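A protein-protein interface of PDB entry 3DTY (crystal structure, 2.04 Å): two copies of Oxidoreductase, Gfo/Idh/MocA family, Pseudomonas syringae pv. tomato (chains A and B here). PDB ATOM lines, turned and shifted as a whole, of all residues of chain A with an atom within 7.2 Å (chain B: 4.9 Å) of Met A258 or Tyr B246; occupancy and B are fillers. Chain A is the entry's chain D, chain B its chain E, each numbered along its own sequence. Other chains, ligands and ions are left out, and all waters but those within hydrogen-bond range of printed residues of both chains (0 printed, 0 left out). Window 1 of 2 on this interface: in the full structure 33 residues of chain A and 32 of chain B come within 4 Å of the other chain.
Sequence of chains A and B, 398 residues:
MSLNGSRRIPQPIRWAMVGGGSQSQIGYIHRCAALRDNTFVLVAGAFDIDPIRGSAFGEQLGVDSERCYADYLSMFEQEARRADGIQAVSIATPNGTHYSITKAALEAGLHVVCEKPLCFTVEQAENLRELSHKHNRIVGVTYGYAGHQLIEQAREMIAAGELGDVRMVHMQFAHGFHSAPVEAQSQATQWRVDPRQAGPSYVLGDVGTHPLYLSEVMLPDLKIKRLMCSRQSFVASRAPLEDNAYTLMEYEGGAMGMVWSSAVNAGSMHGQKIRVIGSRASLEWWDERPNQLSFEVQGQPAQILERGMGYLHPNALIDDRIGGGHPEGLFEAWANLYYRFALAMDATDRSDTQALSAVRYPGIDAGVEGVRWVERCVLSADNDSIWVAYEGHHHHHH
The side-chain amide nitrogen (ND2) of Asn B244 is in hydrogen-bond range of the side-chain sulfur (SD) of Met A168 (3.3 Å).
The side-chain hydroxyl of Tyr B246 lies close to the side-chain sulfur of Met A168 (3.4 Å).
The side-chain sulfur (SD) of Met A228 sits close to the side-chain sulfur (SD) of Met B228, 3.3 Å away.
OH of Tyr B246 sits at hydrogen-bond distance from NE2 of His A170 (2.7 Å).
The backbone NH of Gln B232 lies within hydrogen-bond range of the backbone carbonyl oxygen of Asn B244, at 2.9 Å.
The backbone NH of Met A258 lies within hydrogen-bond range of the backbone carbonyl oxygen of Val A169 (3.0 Å).
The side-chain sulfur (SG) of Cys B229 sits close to the backbone carbonyl oxygen (O) of Tyr B246 (3.5 Å).
N of Arg A167 is in hydrogen-bond range of O of Ile A277 (2.7 Å).
O of Leu A248 lies within hydrogen-bond range of N of Met A228 (2.9 Å).
The backbone carbonyl oxygen (O) of Met A168 is in hydrogen-bond range of the backbone NH (N) of Ile A277 (2.8 Å).
Among the printed residues, pairs that only touch across the chains: His A170 with Trp B260 (3.3 Å), Met A258 with Tyr B246 (3.5 Å), Leu A248 with Ser B230 (3.6 Å), Met A256 with Gln B232 (3.7 Å), Met A256 with Tyr B246 (3.8 Å), Ile A277 with Trp B260 (3.8 Å), Met A256 with Ser B230 (3.8 Å), Leu A248 with Tyr B246 (3.8 Å) and Tyr A246 with Leu B248 (3.9 Å).
Tyr A251 touches none of the printed residues of chain B.
Of the printed residues of chain B, Met A256 touches Ser B230, Gln B232 and Tyr B246.
Of the printed residues of chain B, Met A258 touches Tyr B246 (3.5 Å).
Of the printed residues of chain A, Asn B244 touches Met A168 (3.3 Å).
The nearest printed residue of chain B that does not touch His A170 is Asn B244 (5.5 Å).
Of the 12 printed residues of chain B, 7 touch a printed residue of chain A.
Hydrophobic or aromatic side chains of chain B within 4 Å of the printed part of chain A: Met B228, Tyr B246, Leu B248 and Trp B260.
Of the 22 printed residues of chain A, 8 touch a printed residue of chain B.
Among the printed residues, no Asp or Glu carboxylate lies within 4 Å of a Lys or Arg side-chain nitrogen of the other chain.
Met B228 touches its own counterpart, Met A228.
Tyr A246 touches Leu B248, and with the chains exchanged Leu A248 touches Tyr B246.
Met A258 touches Tyr B246, but with the chains exchanged Tyr A246 does not touch Met B258 (4.1 Å).
Positions printed for both chains: 228, 245, 246, 247, 248, 258, 259 and 260.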
ATOM      1  N   ARG A 167      -2.305  17.963  -1.177  1.00  0.00           N
ATOM      2  CA  ARG A 167      -3.274  17.070  -1.805  1.00  0.00           C
ATOM      3  C   ARG A 167      -3.579  15.853  -0.953  1.00  0.00           C
ATOM      4  O   ARG A 167      -4.730  15.422  -0.871  1.00  0.00           O
ATOM      5  CB  ARG A 167      -2.775  16.643  -3.190  1.00  0.00           C
ATOM      6  CG  ARG A 167      -2.864  17.780  -4.213  1.00  0.00           C
ATOM      7  CD  ARG A 167      -2.146  17.471  -5.529  1.00  0.00           C
ATOM      8  NE  ARG A 167      -2.458  18.482  -6.546  1.00  0.00           N
ATOM      9  CZ  ARG A 167      -1.928  18.510  -7.763  1.00  0.00           C
ATOM     10  NH1 ARG A 167      -1.050  17.586  -8.127  1.00  0.00           N
ATOM     11  NH2 ARG A 167      -2.291  19.451  -8.628  1.00  0.00           N
ATOM     12  N   MET A 168      -2.556  15.307  -0.306  1.00  0.00           N
ATOM     13  CA  MET A 168      -2.750  14.136   0.540  1.00  0.00           C
ATOM     14  C   MET A 168      -1.909  14.140   1.813  1.00  0.00           C
ATOM     15  O   MET A 168      -0.813  14.705   1.859  1.00  0.00           O
ATOM     16  CB  MET A 168      -2.448  12.857  -0.252  1.00  0.00           C
ATOM     17  CG  MET A 168      -3.432  12.558  -1.368  1.00  0.00           C
ATOM     18  SD  MET A 168      -2.612  11.413  -2.678  1.00  0.00           S
ATOM     19  CE  MET A 168      -1.710  12.818  -3.643  1.00  0.00           C
ATOM     20  N   VAL A 169      -2.450  13.498   2.847  1.00  0.00           N
ATOM     21  CA  VAL A 169      -1.769  13.355   4.122  1.00  0.00           C
ATOM     22  C   VAL A 169      -1.886  11.891   4.511  1.00  0.00           C
ATOM     23  O   VAL A 169      -2.942  11.440   4.961  1.00  0.00           O
ATOM     24  CB  VAL A 169      -2.408  14.176   5.234  1.00  0.00           C
ATOM     25  CG1 VAL A 169      -1.543  14.074   6.487  1.00  0.00           C
ATOM     26  CG2 VAL A 169      -2.567  15.620   4.802  1.00  0.00           C
ATOM     27  N   HIS A 170      -0.799  11.153   4.328  1.00  0.00           N
ATOM     28  CA  HIS A 170      -0.776   9.736   4.646  1.00  0.00           C
ATOM     29  C   HIS A 170      -0.043   9.509   5.944  1.00  0.00           C
ATOM     30  O   HIS A 170       1.114   9.898   6.096  1.00  0.00           O
ATOM     31  CB  HIS A 170      -0.114   8.964   3.510  1.00  0.00           C
ATOM     32  CG  HIS A 170      -0.913   8.970   2.242  1.00  0.00           C
ATOM     33  ND1 HIS A 170      -0.474   8.380   1.081  1.00  0.00           N
ATOM     34  CD2 HIS A 170      -2.138   9.481   1.970  1.00  0.00           C
ATOM     35  CE1 HIS A 170      -1.395   8.526   0.143  1.00  0.00           C
ATOM     36  NE2 HIS A 170      -2.412   9.189   0.658  1.00  0.00           N
ATOM     37  N   MET A 171      -0.732   8.885   6.889  1.00  0.00           N
ATOM     38  CA  MET A 171      -0.159   8.631   8.198  1.00  0.00           C
ATOM     39  C   MET A 171      -0.287   7.169   8.587  1.00  0.00           C
ATOM     40  O   MET A 171      -1.175   6.454   8.120  1.00  0.00           O
ATOM     41  CB  MET A 171      -0.868   9.487   9.247  1.00  0.00           C
ATOM     42  CG  MET A 171      -0.845  10.982   8.992  1.00  0.00           C
ATOM     43  SD  MET A 171      -2.391  11.829   9.779  1.00  0.00           S
ATOM     44  CE  MET A 171      -3.666  11.709   8.304  1.00  0.00           C
ATOM     45  N   GLN A 172       0.614   6.726   9.448  1.00  0.00           N
ATOM     46  CA  GLN A 172       0.564   5.357   9.913  1.00  0.00           C
ATOM     47  C   GLN A 172       1.386   5.214  11.175  1.00  0.00           C
ATOM     48  O   GLN A 172       2.352   5.947  11.389  1.00  0.00           O
ATOM     49  CB  GLN A 172       1.108   4.387   8.858  1.00  0.00           C
ATOM     50  CG  GLN A 172       2.634   4.416   8.722  1.00  0.00           C
ATOM     51  CD  GLN A 172       3.187   3.264   7.901  1.00  0.00           C
ATOM     52  OE1 GLN A 172       2.859   3.109   6.728  1.00  0.00           O
ATOM     53  NE2 GLN A 172       4.036   2.449   8.519  1.00  0.00           N
ATOM     54  N   MET A 228     -14.322   7.603   6.989  1.00  0.00           N
ATOM     55  CA  MET A 228     -14.843   6.257   7.161  1.00  0.00           C
ATOM     56  C   MET A 228     -13.715   5.417   7.752  1.00  0.00           C
ATOM     57  O   MET A 228     -12.539   5.752   7.609  1.00  0.00           O
ATOM     58  CB  MET A 228     -15.330   5.657   5.836  1.00  0.00           C
ATOM     59  CG  MET A 228     -14.350   5.709   4.688  1.00  0.00           C
ATOM     60  SD  MET A 228     -14.976   4.564   3.216  1.00  0.00           S
ATOM     61  CE  MET A 228     -16.627   5.449   2.795  1.00  0.00           C
ATOM     62  N   ALA A 245      -6.595  -1.021  11.898  1.00  0.00           N
ATOM     63  CA  ALA A 245      -7.639  -0.153  11.360  1.00  0.00           C
ATOM     64  C   ALA A 245      -7.157   0.799  10.260  1.00  0.00           C
ATOM     65  O   ALA A 245      -6.026   1.310  10.295  1.00  0.00           O
ATOM     66  CB  ALA A 245      -8.274   0.649  12.489  1.00  0.00           C
ATOM     67  N   TYR A 246      -8.033   1.031   9.288  1.00  0.00           N
ATOM     68  CA  TYR A 246      -7.760   1.933   8.177  1.00  0.00           C
ATOM     69  C   TYR A 246      -8.816   3.026   8.252  1.00  0.00           C
ATOM     70  O   TYR A 246     -10.013   2.730   8.332  1.00  0.00           O
ATOM     71  CB  TYR A 246      -7.910   1.218   6.836  1.00  0.00           C
ATOM     72  CG  TYR A 246      -7.123  -0.057   6.705  1.00  0.00           C
ATOM     73  CD1 TYR A 246      -5.755  -0.029   6.447  1.00  0.00           C
ATOM     74  CD2 TYR A 246      -7.753  -1.296   6.803  1.00  0.00           C
ATOM     75  CE1 TYR A 246      -5.032  -1.203   6.281  1.00  0.00           C
ATOM     76  CE2 TYR A 246      -7.038  -2.476   6.640  1.00  0.00           C
ATOM     77  CZ  TYR A 246      -5.681  -2.422   6.377  1.00  0.00           C
ATOM     78  OH  TYR A 246      -4.976  -3.583   6.192  1.00  0.00           O
ATOM     79  N   THR A 247      -8.370   4.279   8.223  1.00  0.00           N
ATOM     80  CA  THR A 247      -9.265   5.430   8.288  1.00  0.00           C
ATOM     81  C   THR A 247      -9.023   6.339   7.087  1.00  0.00           C
ATOM     82  O   THR A 247      -7.931   6.880   6.927  1.00  0.00           O
ATOM     83  CB  THR A 247      -9.021   6.247   9.575  1.00  0.00           C
ATOM     84  OG1 THR A 247      -9.335   5.444  10.713  1.00  0.00           O
ATOM     85  CG2 THR A 247      -9.875   7.507   9.589  1.00  0.00           C
ATOM     86  N   LEU A 248     -10.041   6.492   6.243  1.00  0.00           N
ATOM     87  CA  LEU A 248      -9.945   7.351   5.062  1.00  0.00           C
ATOM     88  C   LEU A 248     -10.711   8.646   5.350  1.00  0.00           C
ATOM     89  O   LEU A 248     -11.863   8.607   5.780  1.00  0.00           O
ATOM     90  CB  LEU A 248     -10.539   6.647   3.841  1.00  0.00           C
ATOM     91  CG  LEU A 248     -10.469   7.421   2.521  1.00  0.00           C
ATOM     92  CD1 LEU A 248      -9.022   7.761   2.200  1.00  0.00           C
ATOM     93  CD2 LEU A 248     -11.080   6.590   1.406  1.00  0.00           C
ATOM     94  N   MET A 249     -10.071   9.786   5.113  1.00  0.00           N
ATOM     95  CA  MET A 249     -10.689  11.076   5.397  1.00  0.00           C
ATOM     96  C   MET A 249     -10.724  12.047   4.220  1.00  0.00           C
ATOM     97  O   MET A 249      -9.839  12.056   3.366  1.00  0.00           O
ATOM     98  CB  MET A 249      -9.958  11.766   6.564  1.00  0.00           C
ATOM     99  CG  MET A 249      -9.777  10.901   7.809  1.00  0.00           C
ATOM    100  SD  MET A 249      -8.724  11.786   9.200  1.00  0.00           S
ATOM    101  CE  MET A 249      -6.978  11.653   8.400  1.00  0.00           C
ATOM    102  N   TYR A 251     -10.867  16.046   3.525  1.00  0.00           N
ATOM    103  CA  TYR A 251     -10.662  17.338   4.152  1.00  0.00           C
ATOM    104  C   TYR A 251     -11.429  18.400   3.379  1.00  0.00           C
ATOM    105  O   TYR A 251     -11.690  18.246   2.181  1.00  0.00           O
ATOM    106  CB  TYR A 251      -9.180  17.725   4.123  1.00  0.00           C
ATOM    107  CG  TYR A 251      -8.260  16.897   4.978  1.00  0.00           C
ATOM    108  CD1 TYR A 251      -8.291  16.997   6.368  1.00  0.00           C
ATOM    109  CD2 TYR A 251      -7.332  16.029   4.395  1.00  0.00           C
ATOM    110  CE1 TYR A 251      -7.414  16.254   7.159  1.00  0.00           C
ATOM    111  CE2 TYR A 251      -6.459  15.282   5.173  1.00  0.00           C
ATOM    112  CZ  TYR A 251      -6.502  15.399   6.549  1.00  0.00           C
ATOM    113  OH  TYR A 251      -5.639  14.662   7.318  1.00  0.00           O
ATOM    114  N   ALA A 255      -8.478  17.892  -0.205  1.00  0.00           N
ATOM    115  CA  ALA A 255      -7.364  17.021   0.169  1.00  0.00           C
ATOM    116  C   ALA A 255      -7.870  15.719   0.779  1.00  0.00           C
ATOM    117  O   ALA A 255      -8.947  15.682   1.383  1.00  0.00           O
ATOM    118  CB  ALA A 255      -6.451  17.727   1.153  1.00  0.00           C
ATOM    119  N   MET A 256      -7.097  14.651   0.621  1.00  0.00           N
ATOM    120  CA  MET A 256      -7.475  13.360   1.176  1.00  0.00           C
ATOM    121  C   MET A 256      -6.514  12.979   2.290  1.00  0.00           C
ATOM    122  O   MET A 256      -5.369  13.409   2.300  1.00  0.00           O
ATOM    123  CB  MET A 256      -7.456  12.277   0.095  1.00  0.00           C
ATOM    124  CG  MET A 256      -8.348  12.563  -1.083  1.00  0.00           C
ATOM    125  SD  MET A 256     -10.225  12.608  -0.642  1.00  0.00           S
ATOM    126  CE  MET A 256     -10.440  10.919   0.286  1.00  0.00           C
ATOM    127  N   GLY A 257      -6.996  12.173   3.230  1.00  0.00           N
ATOM    128  CA  GLY A 257      -6.165  11.741   4.334  1.00  0.00           C
ATOM    129  C   GLY A 257      -6.384  10.271   4.619  1.00  0.00           C
ATOM    130  O   GLY A 257      -7.507   9.775   4.514  1.00  0.00           O
ATOM    131  N   MET A 258      -5.311   9.569   4.973  1.00  0.00           N
ATOM    132  CA  MET A 258      -5.387   8.145   5.267  1.00  0.00           C
ATOM    133  C   MET A 258      -4.583   7.822   6.525  1.00  0.00           C
ATOM    134  O   MET A 258      -3.462   8.311   6.711  1.00  0.00           O
ATOM    135  CB  MET A 258      -4.858   7.331   4.080  1.00  0.00           C
ATOM    136  CG  MET A 258      -4.849   5.815   4.307  1.00  0.00           C
ATOM    137  SD  MET A 258      -6.627   4.987   4.284  1.00  0.00           S
ATOM    138  CE  MET A 258      -6.881   4.924   2.344  1.00  0.00           C
ATOM    139  N   VAL A 259      -5.164   7.005   7.393  1.00  0.00           N
ATOM    140  CA  VAL A 259      -4.507   6.623   8.635  1.00  0.00           C
ATOM    141  C   VAL A 259      -4.568   5.114   8.854  1.00  0.00           C
ATOM    142  O   VAL A 259      -5.659   4.535   8.947  1.00  0.00           O
ATOM    143  CB  VAL A 259      -5.170   7.300   9.870  1.00  0.00           C
ATOM    144  CG1 VAL A 259      -4.497   6.800  11.158  1.00  0.00           C
ATOM    145  CG2 VAL A 259      -5.080   8.822   9.764  1.00  0.00           C
ATOM    146  N   TRP A 260      -3.399   4.486   8.928  1.00  0.00           N
ATOM    147  CA  TRP A 260      -3.332   3.062   9.176  1.00  0.00           C
ATOM    148  C   TRP A 260      -2.791   2.846  10.582  1.00  0.00           C
ATOM    149  O   TRP A 260      -1.637   3.176  10.874  1.00  0.00           O
ATOM    150  CB  TRP A 260      -2.439   2.361   8.142  1.00  0.00           C
ATOM    151  CG  TRP A 260      -2.135   0.915   8.471  1.00  0.00           C
ATOM    152  CD1 TRP A 260      -2.972   0.016   9.072  1.00  0.00           C
ATOM    153  CD2 TRP A 260      -0.910   0.208   8.211  1.00  0.00           C
ATOM    154  NE1 TRP A 260      -2.347  -1.203   9.204  1.00  0.00           N
ATOM    155  CE2 TRP A 260      -1.081  -1.114   8.685  1.00  0.00           C
ATOM    156  CE3 TRP A 260       0.313   0.564   7.619  1.00  0.00           C
ATOM    157  CZ2 TRP A 260      -0.073  -2.086   8.587  1.00  0.00           C
ATOM    158  CZ3 TRP A 260       1.319  -0.404   7.518  1.00  0.00           C
ATOM    159  CH2 TRP A 260       1.114  -1.715   8.002  1.00  0.00           C
ATOM    160  N   LYS A 273       4.853   6.849  10.606  1.00  0.00           N
ATOM    161  CA  LYS A 273       5.293   7.715   9.528  1.00  0.00           C
ATOM    162  C   LYS A 273       4.193   8.642   9.061  1.00  0.00           C
ATOM    163  O   LYS A 273       3.004   8.345   9.202  1.00  0.00           O
ATOM    164  CB  LYS A 273       5.749   6.884   8.325  1.00  0.00           C
ATOM    165  CG  LYS A 273       6.840   5.876   8.630  1.00  0.00           C
ATOM    166  CD  LYS A 273       7.157   5.021   7.410  1.00  0.00           C
ATOM    167  CE  LYS A 273       8.308   4.061   7.691  1.00  0.00           C
ATOM    168  NZ  LYS A 273       8.626   3.202   6.509  1.00  0.00           N
ATOM    169  N   ILE A 277       1.796  15.154   0.923  1.00  0.00           N
ATOM    170  CA  ILE A 277       1.982  15.305  -0.509  1.00  0.00           C
ATOM    171  C   ILE A 277       1.306  16.542  -1.109  1.00  0.00           C
ATOM    172  O   ILE A 277       0.089  16.710  -1.018  1.00  0.00           O
ATOM    173  CB  ILE A 277       1.479  14.031  -1.223  1.00  0.00           C
ATOM    174  CG1 ILE A 277       2.078  12.802  -0.528  1.00  0.00           C
ATOM    175  CG2 ILE A 277       1.869  14.057  -2.690  1.00  0.00           C
ATOM    176  CD1 ILE A 277       1.506  11.476  -0.967  1.00  0.00           C
ATOM    177  N   TRP A 373     -11.968  11.903  17.054  1.00  0.00           N
ATOM    178  CA  TRP A 373     -11.515  11.147  15.897  1.00  0.00           C
ATOM    179  C   TRP A 373     -11.747   9.655  16.147  1.00  0.00           C
ATOM    180  O   TRP A 373     -12.247   8.932  15.281  1.00  0.00           O
ATOM    181  CB  TRP A 373     -10.035  11.415  15.640  1.00  0.00           C
ATOM    182  CG  TRP A 373      -9.524  10.774  14.393  1.00  0.00           C
ATOM    183  CD1 TRP A 373      -9.718  11.200  13.107  1.00  0.00           C
ATOM    184  CD2 TRP A 373      -8.752   9.578  14.307  1.00  0.00           C
ATOM    185  NE1 TRP A 373      -9.115  10.339  12.227  1.00  0.00           N
ATOM    186  CE2 TRP A 373      -8.514   9.333  12.935  1.00  0.00           C
ATOM    187  CE3 TRP A 373      -8.233   8.686  15.256  1.00  0.00           C
ATOM    188  CZ2 TRP A 373      -7.779   8.229  12.487  1.00  0.00           C
ATOM    189  CZ3 TRP A 373      -7.503   7.593  14.815  1.00  0.00           C
ATOM    190  CH2 TRP A 373      -7.283   7.372  13.438  1.00  0.00           C
ATOM    191  N   MET B 228     -13.965  -1.427  -1.849  1.00  0.00           N
ATOM    192  CA  MET B 228     -14.469  -0.076  -1.983  1.00  0.00           C
ATOM    193  C   MET B 228     -13.304   0.739  -2.508  1.00  0.00           C
ATOM    194  O   MET B 228     -12.140   0.455  -2.214  1.00  0.00           O
ATOM    195  CB  MET B 228     -14.976   0.494  -0.657  1.00  0.00           C
ATOM    196  CG  MET B 228     -14.011   0.443   0.485  1.00  0.00           C
ATOM    197  SD  MET B 228     -14.697   1.506   1.972  1.00  0.00           S
ATOM    198  CE  MET B 228     -16.451   0.793   2.212  1.00  0.00           C
ATOM    199  N   CYS B 229     -13.624   1.747  -3.300  1.00  0.00           N
ATOM    200  CA  CYS B 229     -12.604   2.587  -3.882  1.00  0.00           C
ATOM    201  C   CYS B 229     -13.011   4.052  -3.823  1.00  0.00           C
ATOM    202  O   CYS B 229     -14.177   4.402  -4.002  1.00  0.00           O
ATOM    203  CB  CYS B 229     -12.370   2.178  -5.339  1.00  0.00           C
ATOM    204  SG  CYS B 229     -11.149   3.187  -6.217  1.00  0.00           S
ATOM    205  N   SER B 230     -12.027   4.892  -3.543  1.00  0.00           N
ATOM    206  CA  SER B 230     -12.207   6.328  -3.495  1.00  0.00           C
ATOM    207  C   SER B 230     -11.200   6.882  -4.498  1.00  0.00           C
ATOM    208  O   SER B 230     -10.001   6.638  -4.375  1.00  0.00           O
ATOM    209  CB  SER B 230     -11.893   6.858  -2.096  1.00  0.00           C
ATOM    210  OG  SER B 230     -11.823   8.269  -2.115  1.00  0.00           O
ATOM    211  N   GLN B 232      -9.786  10.307  -7.006  1.00  0.00           N
ATOM    212  CA  GLN B 232      -9.789  11.748  -7.208  1.00  0.00           C
ATOM    213  C   GLN B 232      -9.070  12.156  -8.485  1.00  0.00           C
ATOM    214  O   GLN B 232      -8.244  11.413  -9.021  1.00  0.00           O
ATOM    215  CB  GLN B 232      -9.091  12.463  -6.041  1.00  0.00           C
ATOM    216  CG  GLN B 232      -9.575  12.112  -4.641  1.00  0.00           C
ATOM    217  CD  GLN B 232      -9.110  10.744  -4.170  1.00  0.00           C
ATOM    218  OE1 GLN B 232      -7.938  10.381  -4.318  1.00  0.00           O
ATOM    219  NE2 GLN B 232     -10.022   9.984  -3.587  1.00  0.00           N
ATOM    220  N   ASN B 244      -5.400   9.625  -8.822  1.00  0.00           N
ATOM    221  CA  ASN B 244      -5.147   9.105  -7.483  1.00  0.00           C
ATOM    222  C   ASN B 244      -6.328   8.271  -7.004  1.00  0.00           C
ATOM    223  O   ASN B 244      -7.484   8.617  -7.257  1.00  0.00           O
ATOM    224  CB  ASN B 244      -4.896  10.233  -6.476  1.00  0.00           C
ATOM    225  CG  ASN B 244      -4.374   9.709  -5.148  1.00  0.00           C
ATOM    226  OD1 ASN B 244      -5.086   9.700  -4.138  1.00  0.00           O
ATOM    227  ND2 ASN B 244      -3.128   9.253  -5.147  1.00  0.00           N
ATOM    228  N   ALA B 245      -6.047   7.167  -6.322  1.00  0.00           N
ATOM    229  CA  ALA B 245      -7.127   6.337  -5.809  1.00  0.00           C
ATOM    230  C   ALA B 245      -6.702   5.434  -4.667  1.00  0.00           C
ATOM    231  O   ALA B 245      -5.541   5.020  -4.566  1.00  0.00           O
ATOM    232  CB  ALA B 245      -7.739   5.495  -6.932  1.00  0.00           C
ATOM    233  N   TYR B 246      -7.664   5.148  -3.801  1.00  0.00           N
ATOM    234  CA  TYR B 246      -7.451   4.273  -2.668  1.00  0.00           C
ATOM    235  C   TYR B 246      -8.460   3.144  -2.828  1.00  0.00           C
ATOM    236  O   TYR B 246      -9.641   3.391  -3.086  1.00  0.00           O
ATOM    237  CB  TYR B 246      -7.730   4.994  -1.347  1.00  0.00           C
ATOM    238  CG  TYR B 246      -6.932   6.256  -1.115  1.00  0.00           C
ATOM    239  CD1 TYR B 246      -5.600   6.204  -0.708  1.00  0.00           C
ATOM    240  CD2 TYR B 246      -7.507   7.507  -1.322  1.00  0.00           C
ATOM    241  CE1 TYR B 246      -4.857   7.374  -0.513  1.00  0.00           C
ATOM    242  CE2 TYR B 246      -6.780   8.676  -1.134  1.00  0.00           C
ATOM    243  CZ  TYR B 246      -5.458   8.604  -0.732  1.00  0.00           C
ATOM    244  OH  TYR B 246      -4.742   9.763  -0.570  1.00  0.00           O
ATOM    245  N   THR B 247      -7.998   1.912  -2.677  1.00  0.00           N
ATOM    246  CA  THR B 247      -8.873   0.757  -2.774  1.00  0.00           C
ATOM    247  C   THR B 247      -8.697  -0.092  -1.521  1.00  0.00           C
ATOM    248  O   THR B 247      -7.582  -0.501  -1.195  1.00  0.00           O
ATOM    249  CB  THR B 247      -8.549  -0.110  -4.010  1.00  0.00           C
ATOM    250  OG1 THR B 247      -8.654   0.689  -5.196  1.00  0.00           O
ATOM    251  CG2 THR B 247      -9.529  -1.289  -4.111  1.00  0.00           C
ATOM    252  N   LEU B 248      -9.796  -0.323  -0.808  1.00  0.00           N
ATOM    253  CA  LEU B 248      -9.784  -1.143   0.402  1.00  0.00           C
ATOM    254  C   LEU B 248     -10.552  -2.417   0.063  1.00  0.00           C
ATOM    255  O   LEU B 248     -11.665  -2.355  -0.475  1.00  0.00           O
ATOM    256  CB  LEU B 248     -10.460  -0.417   1.564  1.00  0.00           C
ATOM    257  CG  LEU B 248     -10.534  -1.251   2.844  1.00  0.00           C
ATOM    258  CD1 LEU B 248      -9.150  -1.781   3.166  1.00  0.00           C
ATOM    259  CD2 LEU B 248     -11.083  -0.419   3.998  1.00  0.00           C
ATOM    260  N   MET B 258      -5.147  -3.426   0.570  1.00  0.00           N
ATOM    261  CA  MET B 258      -5.211  -2.010   0.254  1.00  0.00           C
ATOM    262  C   MET B 258      -4.312  -1.701  -0.932  1.00  0.00           C
ATOM    263  O   MET B 258      -3.197  -2.218  -1.029  1.00  0.00           O
ATOM    264  CB  MET B 258      -4.779  -1.175   1.464  1.00  0.00           C
ATOM    265  CG  MET B 258      -4.733   0.308   1.178  1.00  0.00           C
ATOM    266  SD  MET B 258      -4.474   1.392   2.767  1.00  0.00           S
ATOM    267  CE  MET B 258      -2.526   1.523   2.726  1.00  0.00           C
ATOM    268  N   VAL B 259      -4.807  -0.872  -1.841  1.00  0.00           N
ATOM    269  CA  VAL B 259      -4.036  -0.480  -3.012  1.00  0.00           C
ATOM    270  C   VAL B 259      -4.126   1.029  -3.197  1.00  0.00           C
ATOM    271  O   VAL B 259      -5.225   1.592  -3.272  1.00  0.00           O
ATOM    272  CB  VAL B 259      -4.566  -1.128  -4.311  1.00  0.00           C
ATOM    273  CG1 VAL B 259      -3.697  -0.701  -5.481  1.00  0.00           C
ATOM    274  CG2 VAL B 259      -4.585  -2.644  -4.186  1.00  0.00           C
ATOM    275  N   TRP B 260      -2.970   1.675  -3.252  1.00  0.00           N
ATOM    276  CA  TRP B 260      -2.908   3.106  -3.466  1.00  0.00           C
ATOM    277  C   TRP B 260      -2.328   3.323  -4.851  1.00  0.00           C
ATOM    278  O   TRP B 260      -1.159   3.018  -5.092  1.00  0.00           O
ATOM    279  CB  TRP B 260      -2.024   3.786  -2.410  1.00  0.00           C
ATOM    280  CG  TRP B 260      -1.761   5.243  -2.701  1.00  0.00           C
ATOM    281  CD1 TRP B 260      -2.638   6.143  -3.234  1.00  0.00           C
ATOM    282  CD2 TRP B 260      -0.539   5.959  -2.478  1.00  0.00           C
ATOM    283  NE1 TRP B 260      -2.037   7.376  -3.359  1.00  0.00           N
ATOM    284  CE2 TRP B 260      -0.749   7.290  -2.900  1.00  0.00           C
ATOM    285  CE3 TRP B 260       0.714   5.605  -1.957  1.00  0.00           C
ATOM    286  CZ2 TRP B 260       0.247   8.269  -2.826  1.00  0.00           C
ATOM    287  CZ3 TRP B 260       1.712   6.587  -1.878  1.00  0.00           C
ATOM    288  CH2 TRP B 260       1.467   7.902  -2.309  1.00  0.00           C
